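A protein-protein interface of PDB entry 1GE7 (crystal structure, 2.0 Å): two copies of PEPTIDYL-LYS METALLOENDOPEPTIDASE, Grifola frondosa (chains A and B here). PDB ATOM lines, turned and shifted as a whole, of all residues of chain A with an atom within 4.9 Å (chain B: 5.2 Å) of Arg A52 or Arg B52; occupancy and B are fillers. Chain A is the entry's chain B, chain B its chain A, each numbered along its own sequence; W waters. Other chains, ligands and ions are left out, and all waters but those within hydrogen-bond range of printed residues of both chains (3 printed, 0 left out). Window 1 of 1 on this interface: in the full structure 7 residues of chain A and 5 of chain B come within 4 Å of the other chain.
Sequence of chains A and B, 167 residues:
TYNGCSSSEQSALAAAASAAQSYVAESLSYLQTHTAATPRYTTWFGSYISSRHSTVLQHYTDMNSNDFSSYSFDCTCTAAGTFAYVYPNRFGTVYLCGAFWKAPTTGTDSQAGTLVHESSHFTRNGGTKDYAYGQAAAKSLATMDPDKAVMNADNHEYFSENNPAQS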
ATOM      1  N   TYR A  41     -11.613  26.808  33.950  1.00  0.00           N
ATOM      2  CA  TYR A  41     -11.694  26.954  32.500  1.00  0.00           C
ATOM      3  C   TYR A  41     -11.160  25.737  31.750  1.00  0.00           C
ATOM      4  O   TYR A  41     -11.843  25.200  30.877  1.00  0.00           O
ATOM      5  CB  TYR A  41     -10.955  28.214  32.022  1.00  0.00           C
ATOM      6  CG  TYR A  41     -10.968  28.404  30.515  1.00  0.00           C
ATOM      7  CD1 TYR A  41     -11.881  29.269  29.910  1.00  0.00           C
ATOM      8  CD2 TYR A  41     -10.096  27.688  29.693  1.00  0.00           C
ATOM      9  CE1 TYR A  41     -11.925  29.417  28.517  1.00  0.00           C
ATOM     10  CE2 TYR A  41     -10.137  27.822  28.298  1.00  0.00           C
ATOM     11  CZ  TYR A  41     -11.052  28.688  27.722  1.00  0.00           C
ATOM     12  OH  TYR A  41     -11.086  28.821  26.346  1.00  0.00           O
ATOM     13  N   PHE A  45     -13.237  23.674  29.141  1.00  0.00           N
ATOM     14  CA  PHE A  45     -13.019  24.213  27.805  1.00  0.00           C
ATOM     15  C   PHE A  45     -11.660  23.865  27.202  1.00  0.00           C
ATOM     16  O   PHE A  45     -11.354  24.256  26.078  1.00  0.00           O
ATOM     17  CB  PHE A  45     -13.263  25.725  27.802  1.00  0.00           C
ATOM     18  CG  PHE A  45     -14.667  26.114  28.216  1.00  0.00           C
ATOM     19  CD1 PHE A  45     -14.878  27.096  29.187  1.00  0.00           C
ATOM     20  CD2 PHE A  45     -15.776  25.485  27.647  1.00  0.00           C
ATOM     21  CE1 PHE A  45     -16.170  27.442  29.583  1.00  0.00           C
ATOM     22  CE2 PHE A  45     -17.081  25.826  28.041  1.00  0.00           C
ATOM     23  CZ  PHE A  45     -17.276  26.802  29.006  1.00  0.00           C
ATOM     24  N   SER A  47      -7.355  23.474  26.835  1.00  0.00           N
ATOM     25  CA  SER A  47      -6.211  24.380  26.823  1.00  0.00           C
ATOM     26  C   SER A  47      -6.660  25.788  26.473  1.00  0.00           C
ATOM     27  O   SER A  47      -7.471  25.984  25.571  1.00  0.00           O
ATOM     28  CB  SER A  47      -5.161  23.907  25.816  1.00  0.00           C
ATOM     29  OG  SER A  47      -4.712  22.603  26.143  1.00  0.00           O
ATOM     30  N   ILE A  49      -6.512  29.417  24.954  1.00  0.00           N
ATOM     31  CA  ILE A  49      -5.986  30.209  23.839  1.00  0.00           C
ATOM     32  C   ILE A  49      -7.063  31.271  23.623  1.00  0.00           C
ATOM     33  O   ILE A  49      -8.243  31.018  23.877  1.00  0.00           O
ATOM     34  CB  ILE A  49      -5.730  29.417  22.518  1.00  0.00           C
ATOM     35  CG1 ILE A  49      -7.024  28.836  21.951  1.00  0.00           C
ATOM     36  CG2 ILE A  49      -4.668  28.351  22.722  1.00  0.00           C
ATOM     37  CD1 ILE A  49      -6.859  28.297  20.532  1.00  0.00           C
ATOM     38  N   SER A  50      -6.654  32.460  23.196  1.00  0.00           N
ATOM     39  CA  SER A  50      -7.573  33.574  22.986  1.00  0.00           C
ATOM     40  C   SER A  50      -8.842  33.297  22.192  1.00  0.00           C
ATOM     41  O   SER A  50      -9.935  33.622  22.651  1.00  0.00           O
ATOM     42  CB  SER A  50      -6.839  34.761  22.364  1.00  0.00           C
ATOM     43  OG  SER A  50      -5.870  35.265  23.258  1.00  0.00           O
ATOM     44  N   SER A  51      -8.694  32.719  21.002  1.00  0.00           N
ATOM     45  CA  SER A  51      -9.836  32.423  20.135  1.00  0.00           C
ATOM     46  C   SER A  51     -10.912  31.562  20.801  1.00  0.00           C
ATOM     47  O   SER A  51     -12.099  31.820  20.625  1.00  0.00           O
ATOM     48  CB  SER A  51      -9.371  31.770  18.833  1.00  0.00           C
ATOM     49  OG  SER A  51      -8.773  30.514  19.085  1.00  0.00           O
ATOM     50  N   ARG A  52     -10.499  30.533  21.541  1.00  0.00           N
ATOM     51  CA  ARG A  52     -11.459  29.671  22.233  1.00  0.00           C
ATOM     52  C   ARG A  52     -12.110  30.420  23.390  1.00  0.00           C
ATOM     53  O   ARG A  52     -13.319  30.326  23.587  1.00  0.00           O
ATOM     54  CB  ARG A  52     -10.793  28.398  22.752  1.00  0.00           C
ATOM     55  CG  ARG A  52     -10.404  27.412  21.659  1.00  0.00           C
ATOM     56  CD  ARG A  52      -9.646  26.231  22.245  1.00  0.00           C
ATOM     57  NE  ARG A  52      -8.872  25.529  21.225  1.00  0.00           N
ATOM     58  CZ  ARG A  52      -7.685  24.977  21.442  1.00  0.00           C
ATOM     59  NH1 ARG A  52      -7.133  25.043  22.649  1.00  0.00           N
ATOM     60  NH2 ARG A  52      -7.043  24.376  20.449  1.00  0.00           N
ATOM     61  N   HIS A  53     -11.308  31.163  24.153  1.00  0.00           N
ATOM     62  CA  HIS A  53     -11.837  31.937  25.277  1.00  0.00           C
ATOM     63  C   HIS A  53     -12.823  32.987  24.762  1.00  0.00           C
ATOM     64  O   HIS A  53     -13.837  33.269  25.401  1.00  0.00           O
ATOM     65  CB  HIS A  53     -10.705  32.607  26.059  1.00  0.00           C
ATOM     66  CG  HIS A  53     -11.180  33.604  27.070  1.00  0.00           C
ATOM     67  ND1 HIS A  53     -11.238  34.954  26.808  1.00  0.00           N
ATOM     68  CD2 HIS A  53     -11.652  33.445  28.328  1.00  0.00           C
ATOM     69  CE1 HIS A  53     -11.728  35.584  27.859  1.00  0.00           C
ATOM     70  NE2 HIS A  53     -11.988  34.690  28.795  1.00  0.00           N
ATOM     71  N   SER A  54     -12.518  33.560  23.602  1.00  0.00           N
ATOM     72  CA  SER A  54     -13.383  34.556  22.986  1.00  0.00           C
ATOM     73  C   SER A  54     -14.729  33.917  22.620  1.00  0.00           C
ATOM     74  O   SER A  54     -15.786  34.532  22.791  1.00  0.00           O
ATOM     75  CB  SER A  54     -12.707  35.138  21.737  1.00  0.00           C
ATOM     76  OG  SER A  54     -13.583  36.000  21.032  1.00  0.00           O
ATOM     77  N   THR A  55     -14.680  32.672  22.147  1.00  0.00           N
ATOM     78  CA  THR A  55     -15.884  31.938  21.770  1.00  0.00           C
ATOM     79  C   THR A  55     -16.831  31.724  22.955  1.00  0.00           C
ATOM     80  O   THR A  55     -18.014  32.067  22.864  1.00  0.00           O
ATOM     81  CB  THR A  55     -15.542  30.578  21.114  1.00  0.00           C
ATOM     82  OG1 THR A  55     -14.876  30.807  19.865  1.00  0.00           O
ATOM     83  CG2 THR A  55     -16.812  29.754  20.859  1.00  0.00           C
ATOM     84  N   VAL A  56     -16.334  31.181  24.067  1.00  0.00           N
ATOM     85  CA  VAL A  56     -17.214  30.977  25.224  1.00  0.00           C
ATOM     86  C   VAL A  56     -17.640  32.296  25.860  1.00  0.00           C
ATOM     87  O   VAL A  56     -18.752  32.407  26.370  1.00  0.00           O
ATOM     88  CB  VAL A  56     -16.617  30.036  26.301  1.00  0.00           C
ATOM     89  CG1 VAL A  56     -16.533  28.623  25.757  1.00  0.00           C
ATOM     90  CG2 VAL A  56     -15.257  30.518  26.752  1.00  0.00           C
ATOM     91  N   MET A 144      -9.367  16.226  24.812  1.00  0.00           N
ATOM     92  CA  MET A 144      -9.123  15.756  23.455  1.00  0.00           C
ATOM     93  C   MET A 144      -9.464  16.729  22.328  1.00  0.00           C
ATOM     94  O   MET A 144      -8.771  16.769  21.313  1.00  0.00           O
ATOM     95  CB  MET A 144      -9.840  14.426  23.225  1.00  0.00           C
ATOM     96  CG  MET A 144      -9.279  13.287  24.058  1.00  0.00           C
ATOM     97  SD  MET A 144     -10.051  11.708  23.671  1.00  0.00           S
ATOM     98  CE  MET A 144      -9.257  11.324  22.125  1.00  0.00           C
ATOM     99  N   PRO A 146     -10.634  20.656  22.377  1.00  0.00           N
ATOM    100  CA  PRO A 146     -11.008  21.949  22.962  1.00  0.00           C
ATOM    101  C   PRO A 146     -12.000  22.702  22.085  1.00  0.00           C
ATOM    102  O   PRO A 146     -12.910  23.348  22.591  1.00  0.00           O
ATOM    103  CB  PRO A 146      -9.674  22.688  23.032  1.00  0.00           C
ATOM    104  CG  PRO A 146      -8.675  21.580  23.187  1.00  0.00           C
ATOM    105  CD  PRO A 146      -9.172  20.559  22.213  1.00  0.00           C
ATOM    106  N   ASP A 147     -11.814  22.618  20.768  1.00  0.00           N
ATOM    107  CA  ASP A 147     -12.701  23.288  19.818  1.00  0.00           C
ATOM    108  C   ASP A 147     -14.130  22.792  19.944  1.00  0.00           C
ATOM    109  O   ASP A 147     -15.074  23.578  19.853  1.00  0.00           O
ATOM    110  CB  ASP A 147     -12.209  23.089  18.385  1.00  0.00           C
ATOM    111  CG  ASP A 147     -10.948  23.875  18.090  1.00  0.00           C
ATOM    112  OD1 ASP A 147     -10.514  24.673  18.945  1.00  0.00           O
ATOM    113  OD2 ASP A 147     -10.393  23.697  16.993  1.00  0.00           O
ATOM    114  N   VAL A 150     -15.755  23.937  23.541  1.00  0.00           N
ATOM    115  CA  VAL A 150     -16.328  25.285  23.593  1.00  0.00           C
ATOM    116  C   VAL A 150     -17.613  25.394  22.770  1.00  0.00           C
ATOM    117  O   VAL A 150     -18.263  26.438  22.752  1.00  0.00           O
ATOM    118  CB  VAL A 150     -15.319  26.384  23.143  1.00  0.00           C
ATOM    119  CG1 VAL A 150     -14.129  26.434  24.107  1.00  0.00           C
ATOM    120  CG2 VAL A 150     -14.856  26.141  21.715  1.00  0.00           C
ATOM    121  N   TYR B  41       1.248  11.389  13.685  1.00  0.00           N
ATOM    122  CA  TYR B  41       0.701  12.708  13.976  1.00  0.00           C
ATOM    123  C   TYR B  41       0.550  12.994  15.469  1.00  0.00           C
ATOM    124  O   TYR B  41       1.045  14.006  15.954  1.00  0.00           O
ATOM    125  CB  TYR B  41      -0.648  12.913  13.277  1.00  0.00           C
ATOM    126  CG  TYR B  41      -1.261  14.266  13.564  1.00  0.00           C
ATOM    127  CD1 TYR B  41      -1.039  15.344  12.717  1.00  0.00           C
ATOM    128  CD2 TYR B  41      -2.005  14.484  14.727  1.00  0.00           C
ATOM    129  CE1 TYR B  41      -1.534  16.612  13.019  1.00  0.00           C
ATOM    130  CE2 TYR B  41      -2.497  15.744  15.040  1.00  0.00           C
ATOM    131  CZ  TYR B  41      -2.258  16.803  14.185  1.00  0.00           C
ATOM    132  OH  TYR B  41      -2.715  18.058  14.512  1.00  0.00           O
ATOM    133  N   PHE B  45       2.181  15.956  17.400  1.00  0.00           N
ATOM    134  CA  PHE B  45       1.262  17.087  17.423  1.00  0.00           C
ATOM    135  C   PHE B  45       0.068  16.926  18.365  1.00  0.00           C
ATOM    136  O   PHE B  45      -0.801  17.797  18.421  1.00  0.00           O
ATOM    137  CB  PHE B  45       0.803  17.415  15.999  1.00  0.00           C
ATOM    138  CG  PHE B  45       1.927  17.818  15.076  1.00  0.00           C
ATOM    139  CD1 PHE B  45       2.061  17.232  13.820  1.00  0.00           C
ATOM    140  CD2 PHE B  45       2.856  18.778  15.466  1.00  0.00           C
ATOM    141  CE1 PHE B  45       3.099  17.594  12.969  1.00  0.00           C
ATOM    142  CE2 PHE B  45       3.902  19.147  14.624  1.00  0.00           C
ATOM    143  CZ  PHE B  45       4.023  18.554  13.371  1.00  0.00           C
ATOM    144  N   GLY B  46       0.045  15.826  19.117  1.00  0.00           N
ATOM    145  CA  GLY B  46      -1.041  15.594  20.057  1.00  0.00           C
ATOM    146  C   GLY B  46      -2.366  15.154  19.452  1.00  0.00           C
ATOM    147  O   GLY B  46      -2.434  14.798  18.272  1.00  0.00           O
ATOM    148  N   SER B  47      -3.416  15.188  20.274  1.00  0.00           N
ATOM    149  CA  SER B  47      -4.763  14.792  19.866  1.00  0.00           C
ATOM    150  C   SER B  47      -5.142  15.466  18.563  1.00  0.00           C
ATOM    151  O   SER B  47      -5.026  16.679  18.427  1.00  0.00           O
ATOM    152  CB  SER B  47      -5.789  15.170  20.940  1.00  0.00           C
ATOM    153  OG  SER B  47      -5.540  14.483  22.150  1.00  0.00           O
ATOM    154  N   ILE B  49      -7.223  17.199  15.859  1.00  0.00           N
ATOM    155  CA  ILE B  49      -8.415  18.033  15.732  1.00  0.00           C
ATOM    156  C   ILE B  49      -8.142  18.838  14.474  1.00  0.00           C
ATOM    157  O   ILE B  49      -6.985  19.146  14.173  1.00  0.00           O
ATOM    158  CB  ILE B  49      -8.686  18.976  16.953  1.00  0.00           C
ATOM    159  CG1 ILE B  49      -7.628  20.076  17.064  1.00  0.00           C
ATOM    160  CG2 ILE B  49      -8.752  18.171  18.244  1.00  0.00           C
ATOM    161  CD1 ILE B  49      -7.972  21.120  18.108  1.00  0.00           C
ATOM    162  N   SER B  50      -9.198  19.143  13.730  1.00  0.00           N
ATOM    163  CA  SER B  50      -9.087  19.883  12.482  1.00  0.00           C
ATOM    164  C   SER B  50      -8.265  21.167  12.497  1.00  0.00           C
ATOM    165  O   SER B  50      -7.426  21.365  11.620  1.00  0.00           O
ATOM    166  CB  SER B  50     -10.481  20.175  11.924  1.00  0.00           C
ATOM    167  OG  SER B  50     -11.148  18.962  11.634  1.00  0.00           O
ATOM    168  N   SER B  51      -8.502  22.032  13.481  1.00  0.00           N
ATOM    169  CA  SER B  51      -7.785  23.307  13.560  1.00  0.00           C
ATOM    170  C   SER B  51      -6.268  23.176  13.699  1.00  0.00           C
ATOM    171  O   SER B  51      -5.522  23.918  13.052  1.00  0.00           O
ATOM    172  CB  SER B  51      -8.350  24.188  14.684  1.00  0.00           C
ATOM    173  OG  SER B  51      -7.995  23.686  15.954  1.00  0.00           O
ATOM    174  N   ARG B  52      -5.811  22.257  14.552  1.00  0.00           N
ATOM    175  CA  ARG B  52      -4.372  22.047  14.734  1.00  0.00           C
ATOM    176  C   ARG B  52      -3.767  21.401  13.497  1.00  0.00           C
ATOM    177  O   ARG B  52      -2.639  21.719  13.105  1.00  0.00           O
ATOM    178  CB  ARG B  52      -4.089  21.169  15.948  1.00  0.00           C
ATOM    179  CG  ARG B  52      -4.268  21.863  17.278  1.00  0.00           C
ATOM    180  CD  ARG B  52      -3.982  20.890  18.411  1.00  0.00           C
ATOM    181  NE  ARG B  52      -4.606  21.335  19.648  1.00  0.00           N
ATOM    182  CZ  ARG B  52      -5.230  20.540  20.507  1.00  0.00           C
ATOM    183  NH1 ARG B  52      -5.320  19.234  20.276  1.00  0.00           N
ATOM    184  NH2 ARG B  52      -5.769  21.061  21.596  1.00  0.00           N
ATOM    185  N   HIS B  53      -4.498  20.453  12.915  1.00  0.00           N
ATOM    186  CA  HIS B  53      -4.036  19.777  11.705  1.00  0.00           C
ATOM    187  C   HIS B  53      -3.897  20.811  10.589  1.00  0.00           C
ATOM    188  O   HIS B  53      -2.945  20.762   9.806  1.00  0.00           O
ATOM    189  CB  HIS B  53      -5.006  18.663  11.298  1.00  0.00           C
ATOM    190  CG  HIS B  53      -4.714  18.075   9.954  1.00  0.00           C
ATOM    191  ND1 HIS B  53      -5.431  18.407   8.827  1.00  0.00           N
ATOM    192  CD2 HIS B  53      -3.779  17.181   9.554  1.00  0.00           C
ATOM    193  CE1 HIS B  53      -4.953  17.745   7.790  1.00  0.00           C
ATOM    194  NE2 HIS B  53      -3.949  16.993   8.204  1.00  0.00           N
ATOM    195  N   SER B  54      -4.846  21.746  10.521  1.00  0.00           N
ATOM    196  CA  SER B  54      -4.791  22.805   9.514  1.00  0.00           C
ATOM    197  C   SER B  54      -3.546  23.661   9.765  1.00  0.00           C
ATOM    198  O   SER B  54      -2.881  24.086   8.826  1.00  0.00           O
ATOM    199  CB  SER B  54      -6.045  23.693   9.568  1.00  0.00           C
ATOM    200  OG  SER B  54      -7.190  23.005   9.087  1.00  0.00           O
ATOM    201  N   THR B  55      -3.241  23.905  11.038  1.00  0.00           N
ATOM    202  CA  THR B  55      -2.075  24.697  11.409  1.00  0.00           C
ATOM    203  C   THR B  55      -0.790  24.054  10.884  1.00  0.00           C
ATOM    204  O   THR B  55      -0.003  24.710  10.200  1.00  0.00           O
ATOM    205  CB  THR B  55      -1.972  24.875  12.939  1.00  0.00           C
ATOM    206  OG1 THR B  55      -3.097  25.624  13.413  1.00  0.00           O
ATOM    207  CG2 THR B  55      -0.687  25.602  13.317  1.00  0.00           C
ATOM    208  N   VAL B  56      -0.586  22.770  11.184  1.00  0.00           N
ATOM    209  CA  VAL B  56       0.622  22.087  10.725  1.00  0.00           C
ATOM    210  C   VAL B  56       0.631  21.923   9.209  1.00  0.00           C
ATOM    211  O   VAL B  56       1.681  22.021   8.584  1.00  0.00           O
ATOM    212  CB  VAL B  56       0.841  20.717  11.422  1.00  0.00           C
ATOM    213  CG1 VAL B  56       1.082  20.927  12.913  1.00  0.00           C
ATOM    214  CG2 VAL B  56      -0.345  19.801  11.210  1.00  0.00           C
ATOM    215  N   LEU B  57      -0.544  21.706   8.622  1.00  0.00           N
ATOM    216  CA  LEU B  57      -0.661  21.564   7.170  1.00  0.00           C
ATOM    217  C   LEU B  57      -0.195  22.853   6.503  1.00  0.00           C
ATOM    218  O   LEU B  57       0.514  22.822   5.498  1.00  0.00           O
ATOM    219  CB  LEU B  57      -2.117  21.276   6.768  1.00  0.00           C
ATOM    220  CG  LEU B  57      -2.454  21.228   5.270  1.00  0.00           C
ATOM    221  CD1 LEU B  57      -1.743  20.073   4.598  1.00  0.00           C
ATOM    222  CD2 LEU B  57      -3.955  21.085   5.089  1.00  0.00           C
ATOM    223  N   PRO B 146      -0.688  20.336  23.236  1.00  0.00           N
ATOM    224  CA  PRO B 146      -0.737  20.230  21.772  1.00  0.00           C
ATOM    225  C   PRO B 146      -0.709  21.567  21.036  1.00  0.00           C
ATOM    226  O   PRO B 146      -0.088  21.671  19.986  1.00  0.00           O
ATOM    227  CB  PRO B 146      -2.051  19.488  21.520  1.00  0.00           C
ATOM    228  CG  PRO B 146      -2.259  18.715  22.768  1.00  0.00           C
ATOM    229  CD  PRO B 146      -1.844  19.659  23.847  1.00  0.00           C
ATOM    230  N   ASP B 147      -1.382  22.582  21.578  1.00  0.00           N
ATOM    231  CA  ASP B 147      -1.392  23.902  20.944  1.00  0.00           C
ATOM    232  C   ASP B 147       0.025  24.456  20.798  1.00  0.00           C
ATOM    233  O   ASP B 147       0.339  25.124  19.815  1.00  0.00           O
ATOM    234  CB  ASP B 147      -2.265  24.886  21.725  1.00  0.00           C
ATOM    235  CG  ASP B 147      -3.739  24.501  21.718  1.00  0.00           C
ATOM    236  OD1 ASP B 147      -4.222  23.921  20.723  1.00  0.00           O
ATOM    237  OD2 ASP B 147      -4.419  24.783  22.722  1.00  0.00           O
ATOM    238  N   VAL B 150       2.145  22.177  18.067  1.00  0.00           N
ATOM    239  CA  VAL B 150       1.988  22.504  16.647  1.00  0.00           C
ATOM    240  C   VAL B 150       2.662  23.838  16.304  1.00  0.00           C
ATOM    241  O   VAL B 150       2.667  24.260  15.148  1.00  0.00           O
ATOM    242  CB  VAL B 150       0.495  22.485  16.185  1.00  0.00           C
ATOM    243  CG1 VAL B 150      -0.113  21.100  16.428  1.00  0.00           C
ATOM    244  CG2 VAL B 150      -0.315  23.557  16.892  1.00  0.00           C
HETATM  245  O   HOH W   1      -6.296  25.283  17.184  1.00  0.00           O
HETATM  246  O   HOH W   2      -2.743  22.655  24.126  1.00  0.00           O
HETATM  247  O   HOH W   3     -10.871  21.650  15.263  1.00  0.00           O
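NH1 of Arg B52 sits at hydrogen-bond distance from O of Ser B47 (3.2 Å). The backbone carbonyl oxygen of Ser B51 is in hydrogen-bond range of the side-chain hydroxyl of Thr B55 (3.0 Å). The side-chain carboxylate of Asp B147 is in salt-bridge range of the guanidinium group of Arg B52, 2.8 Å away. NH1 of Arg A52 lies within hydrogen-bond range of O of Ser A47, 3.1 Å away. The side-chain carboxylate of Asp A147 is in salt-bridge range of the guanidinium group of Arg A52 (2.9 Å).
OG of Ser B51 sits at hydrogen-bond distance from OD2 of Asp A147. The guanidinium group (NH1) of Arg A52 lies within salt-bridge range of the side-chain carboxylate (OD2) of Asp B147, 2.7 Å away.
Arg A52 touches just these residues of chain B: Arg B52 and Asp B147. Arg B52 touches just these residues of chain A: Arg A52 (3.7 Å) and Pro A146 (3.4 Å). Printed residues of chain B within 4 Å of Pro A146: Arg B52. Of the printed residues of chain A, Ser B51 touches Asp A147. Of the printed residues of chain B, Ser A47 touches Asp B147 (3.3 Å). Val A150 touches none of the printed residues of chain B. The nearest residue of chain A that does not touch Arg B52 is Met A144 (4.4 Å).
Water W1 bridges the side-chain hydroxyl (OG) of Ser B51 (2.6 Å) and the guanidinium group (NH2) of Arg A52 (3.5 Å). Water W3 lies within hydrogen-bond range of OD2 of Asp A147 (2.7 Å), N of Ser B51 (3.0 Å) and N of Ser B50 (3.4 Å). Water W2 bridges OG of Ser A47 (2.8 Å) and N of Asp B147 (2.9 Å).
Ser A47 touches Asp B147, but with the chains exchanged Asp A147 does not touch Ser B47 (9.0 Å). Ile A49 touches Asp B147, and with the chains exchanged Asp A147 touches Ile B49. Arg A52 touches its own counterpart, Arg B52. Asp A147 touches Ser B51, but with the chains exchanged Ser A51 does not touch Asp B147 (8.1 Å). 14 positions are printed for both chains. Of the 9 pairs that touch across the chains among the printed residues, 3 have their exchanged pair printed and touching as well.
Among the printed residues, pairs that only touch across the chains: Ser A47 with Asp B147, Ile A49 with Asp B147, Arg A52 with Arg B52, Met A144 with Ser B47, Met A144 with Ile B49, Pro A146 with Arg B52 and Asp A147 with Ile B49.
Printed residues of chain A that touch a printed residue of chain B: Ser A47, Ile A49, Arg A52, Met A144, Pro A146 and Asp A147. Hydrophobic or aromatic side chains of chain A within 4 Å of the printed part of chain B: Ile A49 and Pro A146. Along chain A the printed residues that touch a printed residue of chain B span positions 47 to 147. Of the 16 printed residues of chain B, 5 touch a printed residue of chain A. Among the printed residues, 9 pairs touch across the chains. Among the printed residues, Asp or Glu carboxylates within 4 Å of a Lys or Arg side-chain nitrogen of the other chain: Arg A52 with Asp B147 (2.7 Å).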
